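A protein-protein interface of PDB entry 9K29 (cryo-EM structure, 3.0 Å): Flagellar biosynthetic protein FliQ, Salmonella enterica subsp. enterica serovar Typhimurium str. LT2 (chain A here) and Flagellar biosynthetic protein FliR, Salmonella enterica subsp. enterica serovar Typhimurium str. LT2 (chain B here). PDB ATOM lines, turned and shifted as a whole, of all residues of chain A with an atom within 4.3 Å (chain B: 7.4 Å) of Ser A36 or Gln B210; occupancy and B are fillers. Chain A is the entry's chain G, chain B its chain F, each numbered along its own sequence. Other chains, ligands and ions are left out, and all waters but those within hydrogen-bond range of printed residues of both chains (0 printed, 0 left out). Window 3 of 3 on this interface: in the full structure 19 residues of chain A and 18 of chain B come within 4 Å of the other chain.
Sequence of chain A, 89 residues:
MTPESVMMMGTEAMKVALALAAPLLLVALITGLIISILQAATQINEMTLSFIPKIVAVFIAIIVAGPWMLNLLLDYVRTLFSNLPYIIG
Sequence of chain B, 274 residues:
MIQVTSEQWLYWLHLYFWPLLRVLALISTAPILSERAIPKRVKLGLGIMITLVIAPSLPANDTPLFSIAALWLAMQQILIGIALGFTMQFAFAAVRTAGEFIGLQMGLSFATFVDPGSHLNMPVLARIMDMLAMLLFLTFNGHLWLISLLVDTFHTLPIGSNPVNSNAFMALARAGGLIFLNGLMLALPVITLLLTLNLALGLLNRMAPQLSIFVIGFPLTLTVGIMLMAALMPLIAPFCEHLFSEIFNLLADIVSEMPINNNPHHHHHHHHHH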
ATOM      1  N   GLY A  32      -4.989  11.009  27.489  1.00  0.00           N
ATOM      2  CA  GLY A  32      -4.968  12.262  28.223  1.00  0.00           C
ATOM      3  C   GLY A  32      -3.789  13.133  27.839  1.00  0.00           C
ATOM      4  O   GLY A  32      -3.933  14.344  27.661  1.00  0.00           O
ATOM      5  N   LEU A  33      -2.609  12.524  27.693  1.00  0.00           N
ATOM      6  CA  LEU A  33      -1.437  13.271  27.246  1.00  0.00           C
ATOM      7  C   LEU A  33      -1.648  13.845  25.853  1.00  0.00           C
ATOM      8  O   LEU A  33      -1.286  14.995  25.589  1.00  0.00           O
ATOM      9  CB  LEU A  33      -0.203  12.371  27.267  1.00  0.00           C
ATOM     10  CG  LEU A  33       0.732  12.486  28.470  1.00  0.00           C
ATOM     11  CD1 LEU A  33       2.015  11.711  28.221  1.00  0.00           C
ATOM     12  CD2 LEU A  33       1.035  13.944  28.771  1.00  0.00           C
ATOM     13  N   ILE A  34      -2.227  13.055  24.946  1.00  0.00           N
ATOM     14  CA  ILE A  34      -2.444  13.527  23.581  1.00  0.00           C
ATOM     15  C   ILE A  34      -3.395  14.717  23.573  1.00  0.00           C
ATOM     16  O   ILE A  34      -3.136  15.736  22.921  1.00  0.00           O
ATOM     17  CB  ILE A  34      -2.963  12.382  22.692  1.00  0.00           C
ATOM     18  CG1 ILE A  34      -1.878  11.322  22.494  1.00  0.00           C
ATOM     19  CG2 ILE A  34      -3.434  12.919  21.351  1.00  0.00           C
ATOM     20  CD1 ILE A  34      -0.514  11.891  22.174  1.00  0.00           C
ATOM     21  N   ILE A  35      -4.505  14.611  24.307  1.00  0.00           N
ATOM     22  CA  ILE A  35      -5.467  15.707  24.343  1.00  0.00           C
ATOM     23  C   ILE A  35      -4.853  16.943  24.990  1.00  0.00           C
ATOM     24  O   ILE A  35      -5.062  18.071  24.528  1.00  0.00           O
ATOM     25  CB  ILE A  35      -6.758  15.271  25.058  1.00  0.00           C
ATOM     26  CG1 ILE A  35      -7.417  14.117  24.305  1.00  0.00           C
ATOM     27  CG2 ILE A  35      -7.725  16.436  25.164  1.00  0.00           C
ATOM     28  CD1 ILE A  35      -7.816  14.464  22.890  1.00  0.00           C
ATOM     29  N   SER A  36      -4.083  16.756  26.066  1.00  0.00           N
ATOM     30  CA  SER A  36      -3.459  17.893  26.735  1.00  0.00           C
ATOM     31  C   SER A  36      -2.445  18.586  25.832  1.00  0.00           C
ATOM     32  O   SER A  36      -2.376  19.818  25.803  1.00  0.00           O
ATOM     33  CB  SER A  36      -2.802  17.435  28.035  1.00  0.00           C
ATOM     34  OG  SER A  36      -3.769  17.247  29.053  1.00  0.00           O
ATOM     35  N   ILE A  37      -1.649  17.814  25.088  1.00  0.00           N
ATOM     36  CA  ILE A  37      -0.679  18.415  24.176  1.00  0.00           C
ATOM     37  C   ILE A  37      -1.391  19.142  23.042  1.00  0.00           C
ATOM     38  O   ILE A  37      -0.975  20.231  22.626  1.00  0.00           O
ATOM     39  CB  ILE A  37       0.294  17.344  23.647  1.00  0.00           C
ATOM     40  CG1 ILE A  37       1.156  16.801  24.788  1.00  0.00           C
ATOM     41  CG2 ILE A  37       1.172  17.910  22.544  1.00  0.00           C
ATOM     42  CD1 ILE A  37       1.984  17.858  25.482  1.00  0.00           C
ATOM     43  N   LEU A  38      -2.475  18.557  22.527  1.00  0.00           N
ATOM     44  CA  LEU A  38      -3.244  19.229  21.484  1.00  0.00           C
ATOM     45  C   LEU A  38      -3.825  20.541  21.993  1.00  0.00           C
ATOM     46  O   LEU A  38      -3.854  21.541  21.266  1.00  0.00           O
ATOM     47  CB  LEU A  38      -4.354  18.311  20.975  1.00  0.00           C
ATOM     48  CG  LEU A  38      -3.922  17.207  20.009  1.00  0.00           C
ATOM     49  CD1 LEU A  38      -5.050  16.215  19.788  1.00  0.00           C
ATOM     50  CD2 LEU A  38      -3.463  17.805  18.690  1.00  0.00           C
ATOM     51  N   GLN A  39      -4.300  20.552  23.238  1.00  0.00           N
ATOM     52  CA  GLN A  39      -4.797  21.790  23.831  1.00  0.00           C
ATOM     53  C   GLN A  39      -3.675  22.805  24.014  1.00  0.00           C
ATOM     54  O   GLN A  39      -3.875  24.007  23.805  1.00  0.00           O
ATOM     55  CB  GLN A  39      -5.474  21.493  25.168  1.00  0.00           C
ATOM     56  CG  GLN A  39      -6.903  21.002  25.051  1.00  0.00           C
ATOM     57  CD  GLN A  39      -7.443  20.483  26.368  1.00  0.00           C
ATOM     58  OE1 GLN A  39      -8.411  21.014  26.908  1.00  0.00           O
ATOM     59  NE2 GLN A  39      -6.814  19.438  26.894  1.00  0.00           N
ATOM     60  N   ALA A  40      -2.492  22.341  24.424  1.00  0.00           N
ATOM     61  CA  ALA A  40      -1.365  23.243  24.644  1.00  0.00           C
ATOM     62  C   ALA A  40      -0.901  23.884  23.343  1.00  0.00           C
ATOM     63  O   ALA A  40      -0.530  25.063  23.324  1.00  0.00           O
ATOM     64  CB  ALA A  40      -0.215  22.494  25.315  1.00  0.00           C
ATOM     65  N   ILE A  44      -7.184  26.476  23.378  1.00  0.00           N
ATOM     66  CA  ILE A  44      -8.357  25.930  24.051  1.00  0.00           C
ATOM     67  C   ILE A  44      -7.929  25.251  25.344  1.00  0.00           C
ATOM     68  O   ILE A  44      -6.888  24.585  25.398  1.00  0.00           O
ATOM     69  CB  ILE A  44      -9.106  24.960  23.120  1.00  0.00           C
ATOM     70  CG1 ILE A  44      -8.226  23.767  22.751  1.00  0.00           C
ATOM     71  CG2 ILE A  44      -9.527  25.669  21.849  1.00  0.00           C
ATOM     72  CD1 ILE A  44      -8.969  22.665  22.032  1.00  0.00           C
ATOM     73  N   ASN A  45      -8.717  25.434  26.402  1.00  0.00           N
ATOM     74  CA  ASN A  45      -8.375  24.858  27.701  1.00  0.00           C
ATOM     75  C   ASN A  45      -9.607  24.734  28.588  1.00  0.00           C
ATOM     76  O   ASN A  45     -10.164  25.743  29.027  1.00  0.00           O
ATOM     77  CB  ASN A  45      -7.277  25.689  28.387  1.00  0.00           C
ATOM     78  CG  ASN A  45      -7.554  27.186  28.357  1.00  0.00           C
ATOM     79  OD1 ASN A  45      -8.665  27.629  28.071  1.00  0.00           O
ATOM     80  ND2 ASN A  45      -6.528  27.975  28.659  1.00  0.00           N
ATOM     81  N   LEU B 204       5.245  19.481  36.245  1.00  0.00           N
ATOM     82  CA  LEU B 204       4.647  19.437  34.915  1.00  0.00           C
ATOM     83  C   LEU B 204       3.496  20.426  34.779  1.00  0.00           C
ATOM     84  O   LEU B 204       3.334  21.037  33.718  1.00  0.00           O
ATOM     85  CB  LEU B 204       4.157  18.024  34.592  1.00  0.00           C
ATOM     86  CG  LEU B 204       5.219  16.925  34.552  1.00  0.00           C
ATOM     87  CD1 LEU B 204       4.630  15.636  34.001  1.00  0.00           C
ATOM     88  CD2 LEU B 204       6.419  17.367  33.731  1.00  0.00           C
ATOM     89  N   ASN B 205       2.692  20.581  35.830  1.00  0.00           N
ATOM     90  CA  ASN B 205       1.638  21.590  35.845  1.00  0.00           C
ATOM     91  C   ASN B 205       2.214  22.995  35.714  1.00  0.00           C
ATOM     92  O   ASN B 205       1.557  23.887  35.166  1.00  0.00           O
ATOM     93  CB  ASN B 205       0.834  21.462  37.140  1.00  0.00           C
ATOM     94  CG  ASN B 205      -0.446  22.271  37.126  1.00  0.00           C
ATOM     95  OD1 ASN B 205      -0.780  22.916  36.136  1.00  0.00           O
ATOM     96  ND2 ASN B 205      -1.163  22.254  38.241  1.00  0.00           N
ATOM     97  N   MET B 207       4.719  24.143  33.790  1.00  0.00           N
ATOM     98  CA  MET B 207       4.930  24.567  32.410  1.00  0.00           C
ATOM     99  C   MET B 207       3.618  24.609  31.639  1.00  0.00           C
ATOM    100  O   MET B 207       3.482  25.372  30.675  1.00  0.00           O
ATOM    101  CB  MET B 207       5.938  23.645  31.723  1.00  0.00           C
ATOM    102  CG  MET B 207       5.476  22.207  31.570  1.00  0.00           C
ATOM    103  SD  MET B 207       6.749  21.152  30.849  1.00  0.00           S
ATOM    104  CE  MET B 207       7.883  21.004  32.227  1.00  0.00           C
ATOM    105  N   ALA B 208       2.644  23.803  32.045  1.00  0.00           N
ATOM    106  CA  ALA B 208       1.348  23.792  31.384  1.00  0.00           C
ATOM    107  C   ALA B 208       0.234  23.656  32.413  1.00  0.00           C
ATOM    108  O   ALA B 208       0.025  22.567  32.962  1.00  0.00           O
ATOM    109  CB  ALA B 208       1.273  22.657  30.363  1.00  0.00           C
ATOM    110  N   PRO B 209      -0.497  24.734  32.707  1.00  0.00           N
ATOM    111  CA  PRO B 209      -1.657  24.607  33.602  1.00  0.00           C
ATOM    112  C   PRO B 209      -2.743  23.711  33.043  1.00  0.00           C
ATOM    113  O   PRO B 209      -3.599  23.244  33.805  1.00  0.00           O
ATOM    114  CB  PRO B 209      -2.144  26.054  33.757  1.00  0.00           C
ATOM    115  CG  PRO B 209      -1.634  26.755  32.541  1.00  0.00           C
ATOM    116  CD  PRO B 209      -0.314  26.114  32.229  1.00  0.00           C
ATOM    117  N   GLN B 210      -2.739  23.460  31.732  1.00  0.00           N
ATOM    118  CA  GLN B 210      -3.737  22.583  31.135  1.00  0.00           C
ATOM    119  C   GLN B 210      -3.585  21.148  31.617  1.00  0.00           C
ATOM    120  O   GLN B 210      -4.578  20.415  31.697  1.00  0.00           O
ATOM    121  CB  GLN B 210      -3.636  22.648  29.615  1.00  0.00           C
ATOM    122  CG  GLN B 210      -4.016  23.995  29.037  1.00  0.00           C
ATOM    123  CD  GLN B 210      -3.881  24.017  27.538  1.00  0.00           C
ATOM    124  OE1 GLN B 210      -3.438  23.040  26.941  1.00  0.00           O
ATOM    125  NE2 GLN B 210      -4.257  25.128  26.918  1.00  0.00           N
ATOM    126  N   LEU B 211      -2.362  20.721  31.923  1.00  0.00           N
ATOM    127  CA  LEU B 211      -2.175  19.429  32.567  1.00  0.00           C
ATOM    128  C   LEU B 211      -2.859  19.446  33.927  1.00  0.00           C
ATOM    129  O   LEU B 211      -2.642  20.357  34.731  1.00  0.00           O
ATOM    130  CB  LEU B 211      -0.690  19.106  32.726  1.00  0.00           C
ATOM    131  CG  LEU B 211       0.256  19.307  31.541  1.00  0.00           C
ATOM    132  CD1 LEU B 211       1.611  18.689  31.841  1.00  0.00           C
ATOM    133  CD2 LEU B 211      -0.324  18.710  30.275  1.00  0.00           C
ATOM    134  N   SER B 212      -3.683  18.438  34.184  1.00  0.00           N
ATOM    135  CA  SER B 212      -4.461  18.374  35.408  1.00  0.00           C
ATOM    136  C   SER B 212      -4.181  17.058  36.112  1.00  0.00           C
ATOM    137  O   SER B 212      -3.734  16.084  35.500  1.00  0.00           O
ATOM    138  CB  SER B 212      -5.963  18.517  35.128  1.00  0.00           C
ATOM    139  OG  SER B 212      -6.243  19.747  34.482  1.00  0.00           O
ATOM    140  N   ILE B 213      -4.434  17.044  37.420  1.00  0.00           N
ATOM    141  CA  ILE B 213      -4.238  15.820  38.187  1.00  0.00           C
ATOM    142  C   ILE B 213      -5.194  14.735  37.704  1.00  0.00           C
ATOM    143  O   ILE B 213      -4.796  13.580  37.519  1.00  0.00           O
ATOM    144  CB  ILE B 213      -4.374  16.102  39.698  1.00  0.00           C
ATOM    145  CG1 ILE B 213      -3.932  14.885  40.509  1.00  0.00           C
ATOM    146  CG2 ILE B 213      -5.788  16.544  40.067  1.00  0.00           C
ATOM    147  CD1 ILE B 213      -2.459  14.573  40.383  1.00  0.00           C
ATOM    148  N   VAL B 215      -6.521  14.489  34.666  1.00  0.00           N
ATOM    149  CA  VAL B 215      -6.220  14.093  33.296  1.00  0.00           C
ATOM    150  C   VAL B 215      -5.004  13.178  33.238  1.00  0.00           C
ATOM    151  O   VAL B 215      -5.003  12.176  32.514  1.00  0.00           O
ATOM    152  CB  VAL B 215      -6.025  15.345  32.423  1.00  0.00           C
ATOM    153  CG1 VAL B 215      -5.673  14.952  30.996  1.00  0.00           C
ATOM    154  CG2 VAL B 215      -7.269  16.215  32.457  1.00  0.00           C
ATOM    155  N   ILE B 216      -3.954  13.496  33.995  1.00  0.00           N
ATOM    156  CA  ILE B 216      -2.658  12.855  33.839  1.00  0.00           C
ATOM    157  C   ILE B 216      -2.206  12.151  35.111  1.00  0.00           C
ATOM    158  O   ILE B 216      -1.777  10.993  35.064  1.00  0.00           O
ATOM    159  CB  ILE B 216      -1.595  13.875  33.381  1.00  0.00           C
ATOM    160  CG1 ILE B 216      -1.847  14.277  31.927  1.00  0.00           C
ATOM    161  CG2 ILE B 216      -0.195  13.307  33.541  1.00  0.00           C
ATOM    162  CD1 ILE B 216      -1.846  13.113  30.971  1.00  0.00           C
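Ser A36 touches just these residues of chain B: Gln B210 (3.6 Å), Leu B211 (3.6 Å) and Val B215 (3.6 Å). Ile A37 touches none of the printed residues of chain B. Of the printed residues of chain B, Asn A45 touches Gln B210. Of the printed residues of chain A, Gln B210 touches Ser A36, Gln A39, Ala A40, Ile A44 and Asn A45. Printed residues of chain A within 4 Å of Val B215: Gly A32 (3.8 Å) and Ser A36 (3.6 Å). The nearest residue of chain B that does not touch Ser A36 is Ile B216 (4.6 Å).
Printed residues of chain A that touch a printed residue of chain B: Gly A32, Leu A33, Ser A36, Gln A39, Ala A40, Ile A44 and Asn A45. Among the printed residues, 10 pairs touch across the chains. Among the printed residues, no Asp or Glu carboxylate lies within 4 Å of a Lys or Arg side-chain nitrogen of the other chain.
O of Gly A32 touches CG1 of Val B215 (3.8 Å). Gly A32 touches Ile B216 (C to CD1, 3.7 Å). CD1 of Ile B216 touches N of Leu A33, 3.4 Å away. Ser A36 touches Gln B210 (O to OE1, 3.6 Å). Leu B211 touches Ser A36 (CD2 to CB, 3.6 Å). Ser A36 touches Val B215. CB of Asn A45 touches NE2 of Gln B210, at 3.4 Å.
O of Gly A32 lies within hydrogen-bond range of OG of Ser A36. OD1 of Asn B205 lies close to O of Leu B211, 3.5 Å away. The side-chain hydroxyl (OG) of Ser B212 is in hydrogen-bond range of the backbone carbonyl oxygen (O) of Gln B210 (3.3 Å). NE2 of Gln A39 lies within hydrogen-bond range of O of Ile A35 (3.2 Å).
The backbone carbonyl oxygen (O) of Gln A39 sits close to the side-chain amide oxygen (OE1) of Gln B210, 3.3 Å away. NE2 of Gln B210 sits at hydrogen-bond distance from O of Ile A44, at 3.1 Å. The side-chain amide oxygen (OE1) of Gln B210 is in hydrogen-bond range of the backbone NH (N) of Ala A40 (2.8 Å).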
